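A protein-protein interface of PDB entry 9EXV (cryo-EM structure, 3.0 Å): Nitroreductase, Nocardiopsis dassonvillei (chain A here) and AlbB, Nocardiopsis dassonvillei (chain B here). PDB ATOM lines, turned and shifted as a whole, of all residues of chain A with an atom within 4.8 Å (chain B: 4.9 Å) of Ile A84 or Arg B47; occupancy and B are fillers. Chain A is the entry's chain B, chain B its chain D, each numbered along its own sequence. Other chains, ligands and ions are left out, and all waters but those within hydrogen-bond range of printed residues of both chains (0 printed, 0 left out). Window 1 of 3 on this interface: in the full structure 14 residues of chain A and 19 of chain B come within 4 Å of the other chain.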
ATOM      1  N   LEU A  77      11.086  29.484 -15.236  1.00  0.00           N
ATOM      2  CA  LEU A  77      11.639  30.402 -14.245  1.00  0.00           C
ATOM      3  C   LEU A  77      12.904  29.837 -13.613  1.00  0.00           C
ATOM      4  O   LEU A  77      13.871  30.568 -13.390  1.00  0.00           O
ATOM      5  CB  LEU A  77      10.593  30.717 -13.180  1.00  0.00           C
ATOM      6  CG  LEU A  77       9.628  31.838 -13.562  1.00  0.00           C
ATOM      7  CD1 LEU A  77       8.379  31.795 -12.707  1.00  0.00           C
ATOM      8  CD2 LEU A  77      10.316  33.188 -13.433  1.00  0.00           C
ATOM      9  N   ARG A  78      12.912  28.537 -13.314  1.00  0.00           N
ATOM     10  CA  ARG A  78      14.118  27.920 -12.774  1.00  0.00           C
ATOM     11  C   ARG A  78      15.268  28.003 -13.768  1.00  0.00           C
ATOM     12  O   ARG A  78      16.410  28.286 -13.389  1.00  0.00           O
ATOM     13  CB  ARG A  78      13.843  26.466 -12.396  1.00  0.00           C
ATOM     14  CG  ARG A  78      15.044  25.745 -11.809  1.00  0.00           C
ATOM     15  CD  ARG A  78      14.700  24.308 -11.471  1.00  0.00           C
ATOM     16  NE  ARG A  78      15.841  23.577 -10.936  1.00  0.00           N
ATOM     17  CZ  ARG A  78      16.734  22.933 -11.675  1.00  0.00           C
ATOM     18  NH1 ARG A  78      16.663  22.930 -12.997  1.00  0.00           N
ATOM     19  NH2 ARG A  78      17.721  22.275 -11.075  1.00  0.00           N
ATOM     20  N   SER A  81      16.425  31.584 -13.757  1.00  0.00           N
ATOM     21  CA  SER A  81      16.803  32.100 -12.443  1.00  0.00           C
ATOM     22  C   SER A  81      17.865  31.181 -11.859  1.00  0.00           C
ATOM     23  O   SER A  81      17.540  30.170 -11.222  1.00  0.00           O
ATOM     24  CB  SER A  81      15.592  32.209 -11.518  1.00  0.00           C
ATOM     25  OG  SER A  81      15.965  32.706 -10.250  1.00  0.00           O
ATOM     26  N   PRO A  82      19.149  31.491 -12.060  1.00  0.00           N
ATOM     27  CA  PRO A  82      20.203  30.623 -11.512  1.00  0.00           C
ATOM     28  C   PRO A  82      20.180  30.522  -9.999  1.00  0.00           C
ATOM     29  O   PRO A  82      20.719  29.552  -9.452  1.00  0.00           O
ATOM     30  CB  PRO A  82      21.498  31.276 -12.013  1.00  0.00           C
ATOM     31  CG  PRO A  82      21.131  32.689 -12.296  1.00  0.00           C
ATOM     32  CD  PRO A  82      19.709  32.653 -12.773  1.00  0.00           C
ATOM     33  N   GLY A  83      19.577  31.489  -9.306  1.00  0.00           N
ATOM     34  CA  GLY A  83      19.499  31.402  -7.857  1.00  0.00           C
ATOM     35  C   GLY A  83      18.732  30.182  -7.387  1.00  0.00           C
ATOM     36  O   GLY A  83      19.078  29.571  -6.373  1.00  0.00           O
ATOM     37  N   ILE A  84      17.682  29.809  -8.119  1.00  0.00           N
ATOM     38  CA  ILE A  84      16.883  28.647  -7.754  1.00  0.00           C
ATOM     39  C   ILE A  84      17.702  27.382  -7.967  1.00  0.00           C
ATOM     40  O   ILE A  84      18.322  27.194  -9.021  1.00  0.00           O
ATOM     41  CB  ILE A  84      15.579  28.618  -8.565  1.00  0.00           C
ATOM     42  CG1 ILE A  84      14.753  29.871  -8.275  1.00  0.00           C
ATOM     43  CG2 ILE A  84      14.780  27.361  -8.250  1.00  0.00           C
ATOM     44  CD1 ILE A  84      13.586  30.078  -9.214  1.00  0.00           C
ATOM     45  N   ILE A  85      17.712  26.512  -6.961  1.00  0.00           N
ATOM     46  CA  ILE A  85      18.549  25.316  -6.986  1.00  0.00           C
ATOM     47  C   ILE A  85      17.793  24.116  -7.541  1.00  0.00           C
ATOM     48  O   ILE A  85      18.281  23.424  -8.440  1.00  0.00           O
ATOM     49  CB  ILE A  85      19.104  25.035  -5.575  1.00  0.00           C
ATOM     50  CG1 ILE A  85      19.977  26.200  -5.101  1.00  0.00           C
ATOM     51  CG2 ILE A  85      19.888  23.734  -5.553  1.00  0.00           C
ATOM     52  CD1 ILE A  85      21.264  26.377  -5.889  1.00  0.00           C
ATOM     53  N   GLU A  86      16.598  23.845  -7.024  1.00  0.00           N
ATOM     54  CA  GLU A  86      15.789  22.719  -7.465  1.00  0.00           C
ATOM     55  C   GLU A  86      14.390  23.208  -7.811  1.00  0.00           C
ATOM     56  O   GLU A  86      13.963  24.283  -7.380  1.00  0.00           O
ATOM     57  CB  GLU A  86      15.723  21.617  -6.396  1.00  0.00           C
ATOM     58  CG  GLU A  86      15.063  20.326  -6.861  1.00  0.00           C
ATOM     59  CD  GLU A  86      15.151  19.219  -5.836  1.00  0.00           C
ATOM     60  OE1 GLU A  86      15.767  19.441  -4.773  1.00  0.00           O
ATOM     61  OE2 GLU A  86      14.606  18.125  -6.090  1.00  0.00           O
ATOM     62  N   PRO A  88      10.854  24.236  -7.765  1.00  0.00           N
ATOM     63  CA  PRO A  88       9.996  24.501  -6.616  1.00  0.00           C
ATOM     64  C   PRO A  88       8.537  24.255  -6.951  1.00  0.00           C
ATOM     65  O   PRO A  88       8.088  24.550  -8.068  1.00  0.00           O
ATOM     66  CB  PRO A  88      10.258  25.985  -6.322  1.00  0.00           C
ATOM     67  CG  PRO A  88      10.791  26.563  -7.623  1.00  0.00           C
ATOM     68  CD  PRO A  88      11.002  25.437  -8.605  1.00  0.00           C
ATOM     69  N   SER A 143      15.786  34.613  -3.562  1.00  0.00           N
ATOM     70  CA  SER A 143      16.935  34.748  -4.443  1.00  0.00           C
ATOM     71  C   SER A 143      16.820  36.047  -5.223  1.00  0.00           C
ATOM     72  O   SER A 143      15.730  36.422  -5.661  1.00  0.00           O
ATOM     73  CB  SER A 143      17.042  33.562  -5.410  1.00  0.00           C
ATOM     74  OG  SER A 143      15.921  33.510  -6.275  1.00  0.00           O
ATOM     75  N   LEU A 166      12.830  36.406  -6.275  1.00  0.00           N
ATOM     76  CA  LEU A 166      12.152  35.158  -6.594  1.00  0.00           C
ATOM     77  C   LEU A 166      12.264  34.226  -5.397  1.00  0.00           C
ATOM     78  O   LEU A 166      13.370  33.966  -4.913  1.00  0.00           O
ATOM     79  CB  LEU A 166      12.748  34.500  -7.840  1.00  0.00           C
ATOM     80  CG  LEU A 166      12.142  34.961  -9.165  1.00  0.00           C
ATOM     81  CD1 LEU A 166      12.496  36.412  -9.444  1.00  0.00           C
ATOM     82  CD2 LEU A 166      12.586  34.064 -10.308  1.00  0.00           C
ATOM     83  N   PRO A 168      11.438  30.584  -4.342  1.00  0.00           N
ATOM     84  CA  PRO A 168      11.008  29.179  -4.434  1.00  0.00           C
ATOM     85  C   PRO A 168      10.527  28.663  -3.087  1.00  0.00           C
ATOM     86  O   PRO A 168      11.260  28.677  -2.098  1.00  0.00           O
ATOM     87  CB  PRO A 168      12.280  28.455  -4.897  1.00  0.00           C
ATOM     88  CG  PRO A 168      13.407  29.412  -4.621  1.00  0.00           C
ATOM     89  CD  PRO A 168      12.816  30.765  -4.822  1.00  0.00           C
ATOM     90  N   LEU B  18      18.439  23.541 -19.707  1.00  0.00           N
ATOM     91  CA  LEU B  18      19.775  23.532 -19.119  1.00  0.00           C
ATOM     92  C   LEU B  18      20.691  24.542 -19.799  1.00  0.00           C
ATOM     93  O   LEU B  18      21.479  25.227 -19.134  1.00  0.00           O
ATOM     94  CB  LEU B  18      20.366  22.127 -19.215  1.00  0.00           C
ATOM     95  CG  LEU B  18      21.833  21.959 -18.829  1.00  0.00           C
ATOM     96  CD1 LEU B  18      22.017  22.167 -17.336  1.00  0.00           C
ATOM     97  CD2 LEU B  18      22.330  20.592 -19.260  1.00  0.00           C
ATOM     98  N   TYR B  21      19.870  27.888 -18.563  1.00  0.00           N
ATOM     99  CA  TYR B  21      20.448  28.093 -17.239  1.00  0.00           C
ATOM    100  C   TYR B  21      21.934  28.408 -17.327  1.00  0.00           C
ATOM    101  O   TYR B  21      22.433  29.281 -16.607  1.00  0.00           O
ATOM    102  CB  TYR B  21      20.226  26.871 -16.353  1.00  0.00           C
ATOM    103  CG  TYR B  21      21.215  26.805 -15.210  1.00  0.00           C
ATOM    104  CD1 TYR B  21      21.095  27.646 -14.112  1.00  0.00           C
ATOM    105  CD2 TYR B  21      22.279  25.912 -15.237  1.00  0.00           C
ATOM    106  CE1 TYR B  21      22.001  27.595 -13.069  1.00  0.00           C
ATOM    107  CE2 TYR B  21      23.190  25.855 -14.200  1.00  0.00           C
ATOM    108  CZ  TYR B  21      23.046  26.698 -13.119  1.00  0.00           C
ATOM    109  OH  TYR B  21      23.951  26.644 -12.086  1.00  0.00           O
ATOM    110  N   ASP B  43      26.888  23.370  -9.767  1.00  0.00           N
ATOM    111  CA  ASP B  43      25.434  23.306  -9.880  1.00  0.00           C
ATOM    112  C   ASP B  43      25.018  22.715 -11.218  1.00  0.00           C
ATOM    113  O   ASP B  43      24.184  21.808 -11.282  1.00  0.00           O
ATOM    114  CB  ASP B  43      24.848  24.709  -9.712  1.00  0.00           C
ATOM    115  CG  ASP B  43      23.336  24.707  -9.649  1.00  0.00           C
ATOM    116  OD1 ASP B  43      22.749  23.639  -9.383  1.00  0.00           O
ATOM    117  OD2 ASP B  43      22.732  25.780  -9.865  1.00  0.00           O
ATOM    118  N   ALA B  44      25.597  23.225 -12.303  1.00  0.00           N
ATOM    119  CA  ALA B  44      25.295  22.699 -13.628  1.00  0.00           C
ATOM    120  C   ALA B  44      25.695  21.237 -13.739  1.00  0.00           C
ATOM    121  O   ALA B  44      25.011  20.447 -14.399  1.00  0.00           O
ATOM    122  CB  ALA B  44      26.000  23.533 -14.695  1.00  0.00           C
ATOM    123  N   ALA B  45      26.807  20.860 -13.104  1.00  0.00           N
ATOM    124  CA  ALA B  45      27.249  19.473 -13.144  1.00  0.00           C
ATOM    125  C   ALA B  45      26.235  18.550 -12.487  1.00  0.00           C
ATOM    126  O   ALA B  45      25.912  17.486 -13.026  1.00  0.00           O
ATOM    127  CB  ALA B  45      28.611  19.336 -12.466  1.00  0.00           C
ATOM    128  N   ARG B  46      25.715  18.939 -11.319  1.00  0.00           N
ATOM    129  CA  ARG B  46      24.726  18.093 -10.668  1.00  0.00           C
ATOM    130  C   ARG B  46      23.418  18.062 -11.447  1.00  0.00           C
ATOM    131  O   ARG B  46      22.754  17.023 -11.491  1.00  0.00           O
ATOM    132  CB  ARG B  46      24.490  18.546  -9.223  1.00  0.00           C
ATOM    133  CG  ARG B  46      23.785  19.876  -9.062  1.00  0.00           C
ATOM    134  CD  ARG B  46      23.272  20.065  -7.647  1.00  0.00           C
ATOM    135  NE  ARG B  46      22.040  20.845  -7.634  1.00  0.00           N
ATOM    136  CZ  ARG B  46      20.836  20.343  -7.875  1.00  0.00           C
ATOM    137  NH1 ARG B  46      20.661  19.058  -8.134  1.00  0.00           N
ATOM    138  NH2 ARG B  46      19.782  21.153  -7.862  1.00  0.00           N
ATOM    139  N   ARG B  47      23.037  19.175 -12.077  1.00  0.00           N
ATOM    140  CA  ARG B  47      21.858  19.165 -12.937  1.00  0.00           C
ATOM    141  C   ARG B  47      22.041  18.196 -14.098  1.00  0.00           C
ATOM    142  O   ARG B  47      21.151  17.396 -14.404  1.00  0.00           O
ATOM    143  CB  ARG B  47      21.578  20.577 -13.454  1.00  0.00           C
ATOM    144  CG  ARG B  47      21.087  21.540 -12.388  1.00  0.00           C
ATOM    145  CD  ARG B  47      21.475  22.975 -12.714  1.00  0.00           C
ATOM    146  NE  ARG B  47      20.781  23.933 -11.861  1.00  0.00           N
ATOM    147  CZ  ARG B  47      19.829  24.764 -12.269  1.00  0.00           C
ATOM    148  NH1 ARG B  47      19.442  24.807 -13.533  1.00  0.00           N
ATOM    149  NH2 ARG B  47      19.257  25.577 -11.385  1.00  0.00           N
ATOM    150  N   VAL B  48      23.205  18.253 -14.751  1.00  0.00           N
ATOM    151  CA  VAL B  48      23.479  17.358 -15.871  1.00  0.00           C
ATOM    152  C   VAL B  48      23.484  15.912 -15.405  1.00  0.00           C
ATOM    153  O   VAL B  48      23.019  15.013 -16.116  1.00  0.00           O
ATOM    154  CB  VAL B  48      24.809  17.725 -16.553  1.00  0.00           C
ATOM    155  CG1 VAL B  48      25.161  16.682 -17.605  1.00  0.00           C
ATOM    156  CG2 VAL B  48      24.731  19.097 -17.179  1.00  0.00           C
ATOM    157  N   LEU B  49      24.033  15.656 -14.217  1.00  0.00           N
ATOM    158  CA  LEU B  49      24.084  14.287 -13.723  1.00  0.00           C
ATOM    159  C   LEU B  49      22.697  13.770 -13.368  1.00  0.00           C
ATOM    160  O   LEU B  49      22.404  12.586 -13.565  1.00  0.00           O
ATOM    161  CB  LEU B  49      25.023  14.182 -12.526  1.00  0.00           C
ATOM    162  CG  LEU B  49      26.513  14.191 -12.865  1.00  0.00           C
ATOM    163  CD1 LEU B  49      27.314  14.007 -11.609  1.00  0.00           C
ATOM    164  CD2 LEU B  49      26.862  13.107 -13.877  1.00  0.00           C
ATOM    165  N   ALA B  50      21.829  14.632 -12.834  1.00  0.00           N
ATOM    166  CA  ALA B  50      20.445  14.223 -12.617  1.00  0.00           C
ATOM    167  C   ALA B  50      19.782  13.856 -13.938  1.00  0.00           C
ATOM    168  O   ALA B  50      19.186  12.782 -14.074  1.00  0.00           O
ATOM    169  CB  ALA B  50      19.675  15.338 -11.912  1.00  0.00           C
ATOM    170  N   LEU B  51      19.915  14.725 -14.940  1.00  0.00           N
ATOM    171  CA  LEU B  51      19.329  14.443 -16.243  1.00  0.00           C
ATOM    172  C   LEU B  51      19.892  13.155 -16.832  1.00  0.00           C
ATOM    173  O   LEU B  51      19.144  12.331 -17.374  1.00  0.00           O
ATOM    174  CB  LEU B  51      19.570  15.618 -17.191  1.00  0.00           C
ATOM    175  CG  LEU B  51      19.090  15.393 -18.623  1.00  0.00           C
ATOM    176  CD1 LEU B  51      17.657  14.928 -18.603  1.00  0.00           C
ATOM    177  CD2 LEU B  51      19.239  16.654 -19.457  1.00  0.00           C
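O of Ile A85 lies within hydrogen-bond range of NH2 of Arg A78. The side-chain hydroxyl (OH) of Tyr B21 lies within hydrogen-bond range of the side-chain carboxylate (OD2) of Asp B43. The side-chain carboxylate of Asp B43 is in salt-bridge range of the guanidinium group of Arg B46, 3.4 Å away. OD1 of Asp B43 lies within salt-bridge range of NE of Arg B47 (3.2 Å).
Among the printed residues, merely in contact across the chains: Ile A85 with Arg B47, Pro A82 with Tyr B21 and Arg A78 with Arg B46.
Of chain B, only Arg B47 (3.0 Å) comes within 4 Å of Ile A84. Arg B47 touches just these residues of chain A: Arg A78, Ile A84 and Ile A85. Printed residues of chain A within 4 Å of Tyr B21: Pro A82. Of the printed residues of chain A, Arg B46 touches Arg A78 and Ile A85. Leu A166 touches none of the printed residues of chain B. The nearest residue of chain A that does not touch Arg B47 is Pro A82 (4.7 Å). The nearest printed residue of chain B that does not touch Pro A82 is Asp B43 (4.3 Å).
The backbone carbonyl oxygen (O) of Ile A84 sits at hydrogen-bond distance from the guanidinium group (NH2) of Arg B47 (3.0 Å). The backbone carbonyl oxygen of Ile A85 sits at hydrogen-bond distance from the guanidinium group of Arg B46, 2.8 Å away. NH1 of Arg A78 sits close to NH1 of Arg B47 (3.4 Å).
Printed residues of chain B that touch a printed residue of chain A: Tyr B21, Arg B46 and Arg B47. Printed residues of chain A that touch a printed residue of chain B: Arg A78, Pro A82, Ile A84 and Ile A85. Hydrophobic or aromatic side chains of chain A within 4 Å of the printed part of chain B: Pro A82 and Ile A85.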
